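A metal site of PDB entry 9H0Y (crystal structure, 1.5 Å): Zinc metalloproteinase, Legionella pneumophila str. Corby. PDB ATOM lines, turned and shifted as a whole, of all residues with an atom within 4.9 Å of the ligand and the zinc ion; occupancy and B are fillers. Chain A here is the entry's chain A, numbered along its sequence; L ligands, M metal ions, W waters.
The backbone carbonyl oxygen (O) of Ala 143 lies close to an oxygen (O3) of the ligand. Glu 141 touches the ligand. Met 159 touches the ligand. Tyr 185 touches the ligand (OH to O4, 3.5 Å). Ile 216 touches the ligand. OD2 of Asp 254 touches C3 of the ligand, 3.3 Å away. Tyr 257 touches the ligand. Hydrophobic or aromatic side chains that line the ligand: Met 159, His 170, Ile 216, His 256 and Tyr 257. 14 residues have an atom within 4 Å of the ligand: Glu 141, Asn 142, Ala 143, Met 159, His 170, Glu 171, His 174, Tyr 185, Glu 194, Ile 216, Arg 231, Asp 254, His 256 and Tyr 257. Along chain A the residues within 4 Å of the ligand span positions 141 to 257.
The zinc ion is bound by O4 of the ligand (1.9 Å). OE2 of Glu 194 binds the zinc ion, 2.0 Å away. A ring nitrogen (NE2) of His 174 is bound to the zinc ion, 2.1 Å away. A ring nitrogen (NE2) of His 170 is bound to the zinc ion (2.1 Å).
OD1 of Asn 142 lies within hydrogen-bond range of N2 of the ligand (3.1 Å). An oxygen (O3) of the ligand sits close to the side-chain carboxylate (OE2) of Glu 171. The guanidinium group (NH1) of Arg 231 is in hydrogen-bond range of an oxygen (O5) of the ligand, at 3.0 Å. NE2 of His 256 sits at hydrogen-bond distance from O2 of the ligand, at 3.5 Å.
A ring nitrogen (ND1) of His 256 is in hydrogen-bond range of the side-chain carboxylate (OD2) of Asp 254 (2.7 Å). N of Leu 230 sits at hydrogen-bond distance from O of Ile 216 (2.8 Å). The side-chain hydroxyl of Tyr 185 lies close to a ring nitrogen (NE2) of His 256 (3.3 Å). The side-chain hydroxyl of Tyr 185 lies close to the side-chain carboxylate of Glu 194 (2.7 Å). NH2 of Arg 231 lies within salt-bridge range of OE1 of Glu 194 (3.7 Å). The backbone carbonyl oxygen of His 170 lies within hydrogen-bond range of the side-chain hydroxyl of Ser 197 (2.8 Å). The side-chain carboxylate (OE2) of Glu 141 lies within hydrogen-bond range of the backbone NH (N) of Met 159 (3.1 Å). O of Arg 231 is in hydrogen-bond range of N of Ile 216 (2.9 Å).
Water W3 bridges O2 of the ligand (2.6 Å) and O of Ala 143 (2.7 Å). Water W1 lies within hydrogen-bond range of an oxygen (O2) of the ligand (2.7 Å) and the side-chain amide nitrogen of Asn 142 (2.8 Å). Water W2 bridges an oxygen (O3) of the ligand (2.9 Å) and the side-chain carboxylate of Glu 171 (3.2 Å). Water W4 bridges OH of Tyr 185 (2.7 Å) and O2 of the ligand (2.9 Å).
Tyr 185 touches the zinc ion. The nearest printed residue that does not touch the zinc ion is His 256 (4.1 Å).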
ATOM      1  N   GLU A 141     -33.321  15.411   1.890  1.00  0.00           N
ATOM      2  CA  GLU A 141     -31.936  15.039   2.190  1.00  0.00           C
ATOM      3  C   GLU A 141     -31.853  13.543   2.475  1.00  0.00           C
ATOM      4  O   GLU A 141     -31.448  13.101   3.564  1.00  0.00           O
ATOM      5  CB  GLU A 141     -31.404  15.872   3.346  1.00  0.00           C
ATOM      6  CG  GLU A 141     -31.490  17.383   3.107  1.00  0.00           C
ATOM      7  CD  GLU A 141     -30.549  18.215   3.975  1.00  0.00           C
ATOM      8  OE1 GLU A 141     -30.825  18.287   5.177  1.00  0.00           O
ATOM      9  OE2 GLU A 141     -29.632  18.904   3.445  1.00  0.00           O
ATOM     10  N   ASN A 142     -32.258  12.769   1.481  1.00  0.00           N
ATOM     11  CA  ASN A 142     -32.184  11.319   1.564  1.00  0.00           C
ATOM     12  C   ASN A 142     -32.356  10.719   0.168  1.00  0.00           C
ATOM     13  O   ASN A 142     -32.552  11.424  -0.827  1.00  0.00           O
ATOM     14  CB  ASN A 142     -33.253  10.755   2.506  1.00  0.00           C
ATOM     15  CG  ASN A 142     -32.707   9.666   3.406  1.00  0.00           C
ATOM     16  OD1 ASN A 142     -31.808   8.911   3.025  1.00  0.00           O
ATOM     17  ND2 ASN A 142     -33.301   9.529   4.588  1.00  0.00           N
ATOM     18  N   ALA A 143     -32.291   9.389   0.126  1.00  0.00           N
ATOM     19  CA  ALA A 143     -32.568   8.560  -1.046  1.00  0.00           C
ATOM     20  C   ALA A 143     -33.245   7.298  -0.511  1.00  0.00           C
ATOM     21  O   ALA A 143     -33.151   7.001   0.686  1.00  0.00           O
ATOM     22  CB  ALA A 143     -31.288   8.244  -1.833  1.00  0.00           C
ATOM     23  N   TYR A 144     -33.925   6.561  -1.392  1.00  0.00           N
ATOM     24  CA  TYR A 144     -34.602   5.364  -0.905  1.00  0.00           C
ATOM     25  C   TYR A 144     -34.889   4.391  -2.044  1.00  0.00           C
ATOM     26  O   TYR A 144     -35.023   4.783  -3.216  1.00  0.00           O
ATOM     27  CB  TYR A 144     -35.902   5.710  -0.148  1.00  0.00           C
ATOM     28  CG  TYR A 144     -37.050   6.249  -1.007  1.00  0.00           C
ATOM     29  CD1 TYR A 144     -37.213   7.610  -1.214  1.00  0.00           C
ATOM     30  CD2 TYR A 144     -37.998   5.379  -1.532  1.00  0.00           C
ATOM     31  CE1 TYR A 144     -38.258   8.082  -2.005  1.00  0.00           C
ATOM     32  CE2 TYR A 144     -39.047   5.848  -2.293  1.00  0.00           C
ATOM     33  CZ  TYR A 144     -39.173   7.195  -2.528  1.00  0.00           C
ATOM     34  OH  TYR A 144     -40.228   7.623  -3.296  1.00  0.00           O
ATOM     35  N   MET A 159     -26.711  18.712   2.588  1.00  0.00           N
ATOM     36  CA  MET A 159     -26.275  17.774   1.574  1.00  0.00           C
ATOM     37  C   MET A 159     -26.533  18.333   0.190  1.00  0.00           C
ATOM     38  O   MET A 159     -27.541  19.006  -0.038  1.00  0.00           O
ATOM     39  CB  MET A 159     -27.030  16.447   1.700  1.00  0.00           C
ATOM     40  CG  MET A 159     -26.819  15.768   3.011  1.00  0.00           C
ATOM     41  SD  MET A 159     -27.807  14.287   3.168  1.00  0.00           S
ATOM     42  CE  MET A 159     -27.885  14.210   4.938  1.00  0.00           C
ATOM     43  N   LEU A 162     -28.246  13.890  -3.785  1.00  0.00           N
ATOM     44  CA  LEU A 162     -27.721  12.612  -3.327  1.00  0.00           C
ATOM     45  C   LEU A 162     -27.659  11.611  -4.483  1.00  0.00           C
ATOM     46  O   LEU A 162     -28.250  10.528  -4.457  1.00  0.00           O
ATOM     47  CB  LEU A 162     -28.571  12.082  -2.178  1.00  0.00           C
ATOM     48  CG  LEU A 162     -28.509  12.818  -0.845  1.00  0.00           C
ATOM     49  CD1 LEU A 162     -29.547  13.929  -0.796  1.00  0.00           C
ATOM     50  CD2 LEU A 162     -28.721  11.823   0.290  1.00  0.00           C
ATOM     51  N   VAL A 167     -24.032   6.399  -3.461  1.00  0.00           N
ATOM     52  CA  VAL A 167     -25.425   6.441  -3.038  1.00  0.00           C
ATOM     53  C   VAL A 167     -26.273   5.583  -3.974  1.00  0.00           C
ATOM     54  O   VAL A 167     -27.132   4.825  -3.526  1.00  0.00           O
ATOM     55  CB  VAL A 167     -25.950   7.889  -2.967  1.00  0.00           C
ATOM     56  CG1 VAL A 167     -27.452   7.873  -2.698  1.00  0.00           C
ATOM     57  CG2 VAL A 167     -25.209   8.665  -1.881  1.00  0.00           C
ATOM     58  N   HIS A 170     -25.648   1.910  -3.177  1.00  0.00           N
ATOM     59  CA  HIS A 170     -26.345   1.559  -1.950  1.00  0.00           C
ATOM     60  C   HIS A 170     -27.817   1.296  -2.216  1.00  0.00           C
ATOM     61  O   HIS A 170     -28.369   0.265  -1.791  1.00  0.00           O
ATOM     62  CB  HIS A 170     -26.150   2.686  -0.952  1.00  0.00           C
ATOM     63  CG  HIS A 170     -26.762   2.465   0.381  1.00  0.00           C
ATOM     64  ND1 HIS A 170     -26.030   2.179   1.521  1.00  0.00           N
ATOM     65  CD2 HIS A 170     -28.060   2.410   0.738  1.00  0.00           C
ATOM     66  CE1 HIS A 170     -26.859   2.035   2.526  1.00  0.00           C
ATOM     67  NE2 HIS A 170     -28.089   2.160   2.082  1.00  0.00           N
ATOM     68  N   GLU A 171     -28.483   2.190  -2.953  1.00  0.00           N
ATOM     69  CA  GLU A 171     -29.922   2.045  -3.142  1.00  0.00           C
ATOM     70  C   GLU A 171     -30.253   0.880  -4.068  1.00  0.00           C
ATOM     71  O   GLU A 171     -31.157   0.090  -3.770  1.00  0.00           O
ATOM     72  CB  GLU A 171     -30.529   3.351  -3.662  1.00  0.00           C
ATOM     73  CG  GLU A 171     -30.441   4.520  -2.680  1.00  0.00           C
ATOM     74  CD  GLU A 171     -31.102   4.253  -1.333  1.00  0.00           C
ATOM     75  OE1 GLU A 171     -31.875   3.277  -1.207  1.00  0.00           O
ATOM     76  OE2 GLU A 171     -30.835   5.029  -0.399  1.00  0.00           O
ATOM     77  N   HIS A 174     -30.088  -2.358  -2.162  1.00  0.00           N
ATOM     78  CA  HIS A 174     -31.233  -2.749  -1.328  1.00  0.00           C
ATOM     79  C   HIS A 174     -32.150  -3.665  -2.126  1.00  0.00           C
ATOM     80  O   HIS A 174     -32.708  -4.643  -1.607  1.00  0.00           O
ATOM     81  CB  HIS A 174     -31.988  -1.515  -0.858  1.00  0.00           C
ATOM     82  CG  HIS A 174     -31.475  -0.934   0.404  1.00  0.00           C
ATOM     83  ND1 HIS A 174     -31.179  -1.681   1.535  1.00  0.00           N
ATOM     84  CD2 HIS A 174     -31.190   0.347   0.710  1.00  0.00           C
ATOM     85  CE1 HIS A 174     -30.752  -0.882   2.486  1.00  0.00           C
ATOM     86  NE2 HIS A 174     -30.747   0.355   2.011  1.00  0.00           N
ATOM     87  N   TYR A 185     -35.599  -5.833   7.355  1.00  0.00           N
ATOM     88  CA  TYR A 185     -35.034  -4.504   7.618  1.00  0.00           C
ATOM     89  C   TYR A 185     -35.259  -4.033   9.054  1.00  0.00           C
ATOM     90  O   TYR A 185     -35.813  -2.955   9.301  1.00  0.00           O
ATOM     91  CB  TYR A 185     -35.598  -3.500   6.631  1.00  0.00           C
ATOM     92  CG  TYR A 185     -34.741  -2.287   6.407  1.00  0.00           C
ATOM     93  CD1 TYR A 185     -33.467  -2.393   5.893  1.00  0.00           C
ATOM     94  CD2 TYR A 185     -35.241  -1.014   6.684  1.00  0.00           C
ATOM     95  CE1 TYR A 185     -32.684  -1.267   5.666  1.00  0.00           C
ATOM     96  CE2 TYR A 185     -34.475   0.109   6.470  1.00  0.00           C
ATOM     97  CZ  TYR A 185     -33.203  -0.018   5.963  1.00  0.00           C
ATOM     98  OH  TYR A 185     -32.448   1.115   5.745  1.00  0.00           O
ATOM     99  N   GLU A 194     -28.325  -3.103   5.586  1.00  0.00           N
ATOM    100  CA  GLU A 194     -27.679  -1.804   5.434  1.00  0.00           C
ATOM    101  C   GLU A 194     -26.214  -1.955   5.057  1.00  0.00           C
ATOM    102  O   GLU A 194     -25.720  -1.255   4.166  1.00  0.00           O
ATOM    103  CB  GLU A 194     -27.812  -1.044   6.750  1.00  0.00           C
ATOM    104  CG  GLU A 194     -28.938  -0.052   6.807  1.00  0.00           C
ATOM    105  CD  GLU A 194     -28.994   0.834   5.589  1.00  0.00           C
ATOM    106  OE1 GLU A 194     -28.059   1.645   5.446  1.00  0.00           O
ATOM    107  OE2 GLU A 194     -29.983   0.765   4.827  1.00  0.00           O
ATOM    108  N   SER A 197     -25.446  -2.858   1.438  1.00  0.00           N
ATOM    109  CA  SER A 197     -25.617  -1.697   0.569  1.00  0.00           C
ATOM    110  C   SER A 197     -24.438  -0.735   0.705  1.00  0.00           C
ATOM    111  O   SER A 197     -24.023  -0.134  -0.307  1.00  0.00           O
ATOM    112  CB  SER A 197     -26.962  -1.017   0.882  1.00  0.00           C
ATOM    113  OG  SER A 197     -28.043  -1.679   0.246  1.00  0.00           O
ATOM    114  N   ILE A 216     -19.243   6.617   3.446  1.00  0.00           N
ATOM    115  CA  ILE A 216     -20.528   6.737   2.759  1.00  0.00           C
ATOM    116  C   ILE A 216     -20.905   8.205   2.739  1.00  0.00           C
ATOM    117  O   ILE A 216     -21.010   8.848   3.794  1.00  0.00           O
ATOM    118  CB  ILE A 216     -21.621   5.891   3.428  1.00  0.00           C
ATOM    119  CG1 ILE A 216     -21.194   4.414   3.484  1.00  0.00           C
ATOM    120  CG2 ILE A 216     -22.931   6.053   2.676  1.00  0.00           C
ATOM    121  CD1 ILE A 216     -21.067   3.715   2.150  1.00  0.00           C
ATOM    122  N   LEU A 230     -21.504  10.559   5.914  1.00  0.00           N
ATOM    123  CA  LEU A 230     -22.616   9.910   6.620  1.00  0.00           C
ATOM    124  C   LEU A 230     -22.108   8.796   7.532  1.00  0.00           C
ATOM    125  O   LEU A 230     -22.518   8.707   8.701  1.00  0.00           O
ATOM    126  CB  LEU A 230     -23.622   9.334   5.615  1.00  0.00           C
ATOM    127  CG  LEU A 230     -24.342  10.309   4.691  1.00  0.00           C
ATOM    128  CD1 LEU A 230     -25.215   9.595   3.681  1.00  0.00           C
ATOM    129  CD2 LEU A 230     -25.180  11.266   5.523  1.00  0.00           C
ATOM    130  N   ARG A 231     -21.237   7.928   7.021  1.00  0.00           N
ATOM    131  CA  ARG A 231     -20.738   6.785   7.777  1.00  0.00           C
ATOM    132  C   ARG A 231     -19.282   6.534   7.383  1.00  0.00           C
ATOM    133  O   ARG A 231     -18.843   6.883   6.284  1.00  0.00           O
ATOM    134  CB  ARG A 231     -21.546   5.515   7.499  1.00  0.00           C
ATOM    135  CG  ARG A 231     -22.900   5.482   8.158  1.00  0.00           C
ATOM    136  CD  ARG A 231     -23.704   4.231   7.783  1.00  0.00           C
ATOM    137  NE  ARG A 231     -24.157   4.259   6.391  1.00  0.00           N
ATOM    138  CZ  ARG A 231     -25.318   4.760   5.995  1.00  0.00           C
ATOM    139  NH1 ARG A 231     -26.017   5.572   6.767  1.00  0.00           N
ATOM    140  NH2 ARG A 231     -25.780   4.461   4.783  1.00  0.00           N
ATOM    141  N   ASP A 254     -30.734   1.312  15.654  1.00  0.00           N
ATOM    142  CA  ASP A 254     -31.247   1.354  14.289  1.00  0.00           C
ATOM    143  C   ASP A 254     -30.283   0.671  13.319  1.00  0.00           C
ATOM    144  O   ASP A 254     -29.073   0.611  13.557  1.00  0.00           O
ATOM    145  CB  ASP A 254     -31.464   2.809  13.852  1.00  0.00           C
ATOM    146  CG  ASP A 254     -32.082   2.921  12.488  1.00  0.00           C
ATOM    147  OD1 ASP A 254     -33.301   2.658  12.385  1.00  0.00           O
ATOM    148  OD2 ASP A 254     -31.351   3.245  11.523  1.00  0.00           O
ATOM    149  N   HIS A 256     -29.048   1.638  10.647  1.00  0.00           N
ATOM    150  CA  HIS A 256     -28.020   2.538  10.121  1.00  0.00           C
ATOM    151  C   HIS A 256     -26.842   2.710  11.073  1.00  0.00           C
ATOM    152  O   HIS A 256     -25.857   3.353  10.697  1.00  0.00           O
ATOM    153  CB  HIS A 256     -28.657   3.895   9.807  1.00  0.00           C
ATOM    154  CG  HIS A 256     -29.635   3.826   8.676  1.00  0.00           C
ATOM    155  ND1 HIS A 256     -30.984   3.709   8.876  1.00  0.00           N
ATOM    156  CD2 HIS A 256     -29.447   3.859   7.330  1.00  0.00           C
ATOM    157  CE1 HIS A 256     -31.603   3.645   7.704  1.00  0.00           C
ATOM    158  NE2 HIS A 256     -30.690   3.741   6.759  1.00  0.00           N
ATOM    159  N   TYR A 257     -26.942   2.163  12.276  1.00  0.00           N
ATOM    160  CA  TYR A 257     -25.879   2.160  13.271  1.00  0.00           C
ATOM    161  C   TYR A 257     -25.345   0.758  13.527  1.00  0.00           C
ATOM    162  O   TYR A 257     -24.141   0.573  13.679  1.00  0.00           O
ATOM    163  CB  TYR A 257     -26.412   2.775  14.567  1.00  0.00           C
ATOM    164  CG  TYR A 257     -26.936   4.203  14.377  1.00  0.00           C
ATOM    165  CD1 TYR A 257     -26.248   5.132  13.613  1.00  0.00           C
ATOM    166  CD2 TYR A 257     -28.142   4.593  14.950  1.00  0.00           C
ATOM    167  CE1 TYR A 257     -26.737   6.421  13.433  1.00  0.00           C
ATOM    168  CE2 TYR A 257     -28.636   5.881  14.779  1.00  0.00           C
ATOM    169  CZ  TYR A 257     -27.928   6.791  14.023  1.00  0.00           C
ATOM    170  OH  TYR A 257     -28.399   8.073  13.830  1.00  0.00           O
HETATM  171  C1  LIG L   1     -30.012   7.129  10.287  1.00  0.00           C
HETATM  172  C2  LIG L   1     -30.547   6.822  11.523  1.00  0.00           C
HETATM  173  C3  LIG L   1     -31.883   6.472  11.633  1.00  0.00           C
HETATM  174  C4  LIG L   1     -32.682   6.418  10.505  1.00  0.00           C
HETATM  175  C5  LIG L   1     -32.148   6.725   9.269  1.00  0.00           C
HETATM  176  C6  LIG L   1     -30.813   7.086   9.160  1.00  0.00           C
HETATM  177  C7  LIG L   1     -29.031  10.528   7.022  1.00  0.00           C
HETATM  178  C8  LIG L   1     -29.134  10.504   4.525  1.00  0.00           C
HETATM  179  C9  LIG L   1     -29.199   6.512   4.376  1.00  0.00           C
HETATM  180  C10 LIG L   1     -29.904   5.972   3.134  1.00  0.00           C
HETATM  181  C11 LIG L   1     -28.734   5.596   2.216  1.00  0.00           C
HETATM  182  C12 LIG L   1     -27.714   6.697   1.949  1.00  0.00           C
HETATM  183  C13 LIG L   1     -28.338   7.875   1.235  1.00  0.00           C
HETATM  184  C14 LIG L   1     -26.558   6.101   1.121  1.00  0.00           C
HETATM  185  C15 LIG L   1     -29.420   7.811   7.183  1.00  0.00           C
HETATM  186  C16 LIG L   1     -29.802   8.398   5.818  1.00  0.00           C
HETATM  187  C17 LIG L   1     -29.759   9.944   5.807  1.00  0.00           C
HETATM  188  N1  LIG L   1     -30.514   7.390   7.814  1.00  0.00           N
HETATM  189  N2  LIG L   1     -29.345   7.822   4.578  1.00  0.00           N
HETATM  190  O1  LIG L   1     -28.275   7.888   7.643  1.00  0.00           O
HETATM  191  O2  LIG L   1     -32.273   5.231   4.079  1.00  0.00           O
HETATM  192  O3  LIG L   1     -31.608   4.301   1.816  1.00  0.00           O
HETATM  193  O4  LIG L   1     -30.520   3.475   3.953  1.00  0.00           O
HETATM  194  O5  LIG L   1     -28.459   5.799   5.061  1.00  0.00           O
HETATM  195  P1  LIG L   1     -31.121   4.645   3.238  1.00  0.00           P
HETATM  196 CL1  LIG L   1     -32.547   6.146  13.208  1.00  0.00          CL
HETATM  197 CL2  LIG L   1     -34.331   5.909  10.604  1.00  0.00          CL
HETATM  198 ZN    ZN M   1     -29.857   1.854   3.174  1.00  0.00          ZN
HETATM  199  O   HOH W   1     -32.827   7.107   5.951  1.00  0.00           O
HETATM  200  O   HOH W   2     -34.021   2.914   1.188  1.00  0.00           O
HETATM  201  O   HOH W   3     -34.427   6.073   2.935  1.00  0.00           O
HETATM  202  O   HOH W   4     -33.940   3.303   5.414  1.00  0.00           O
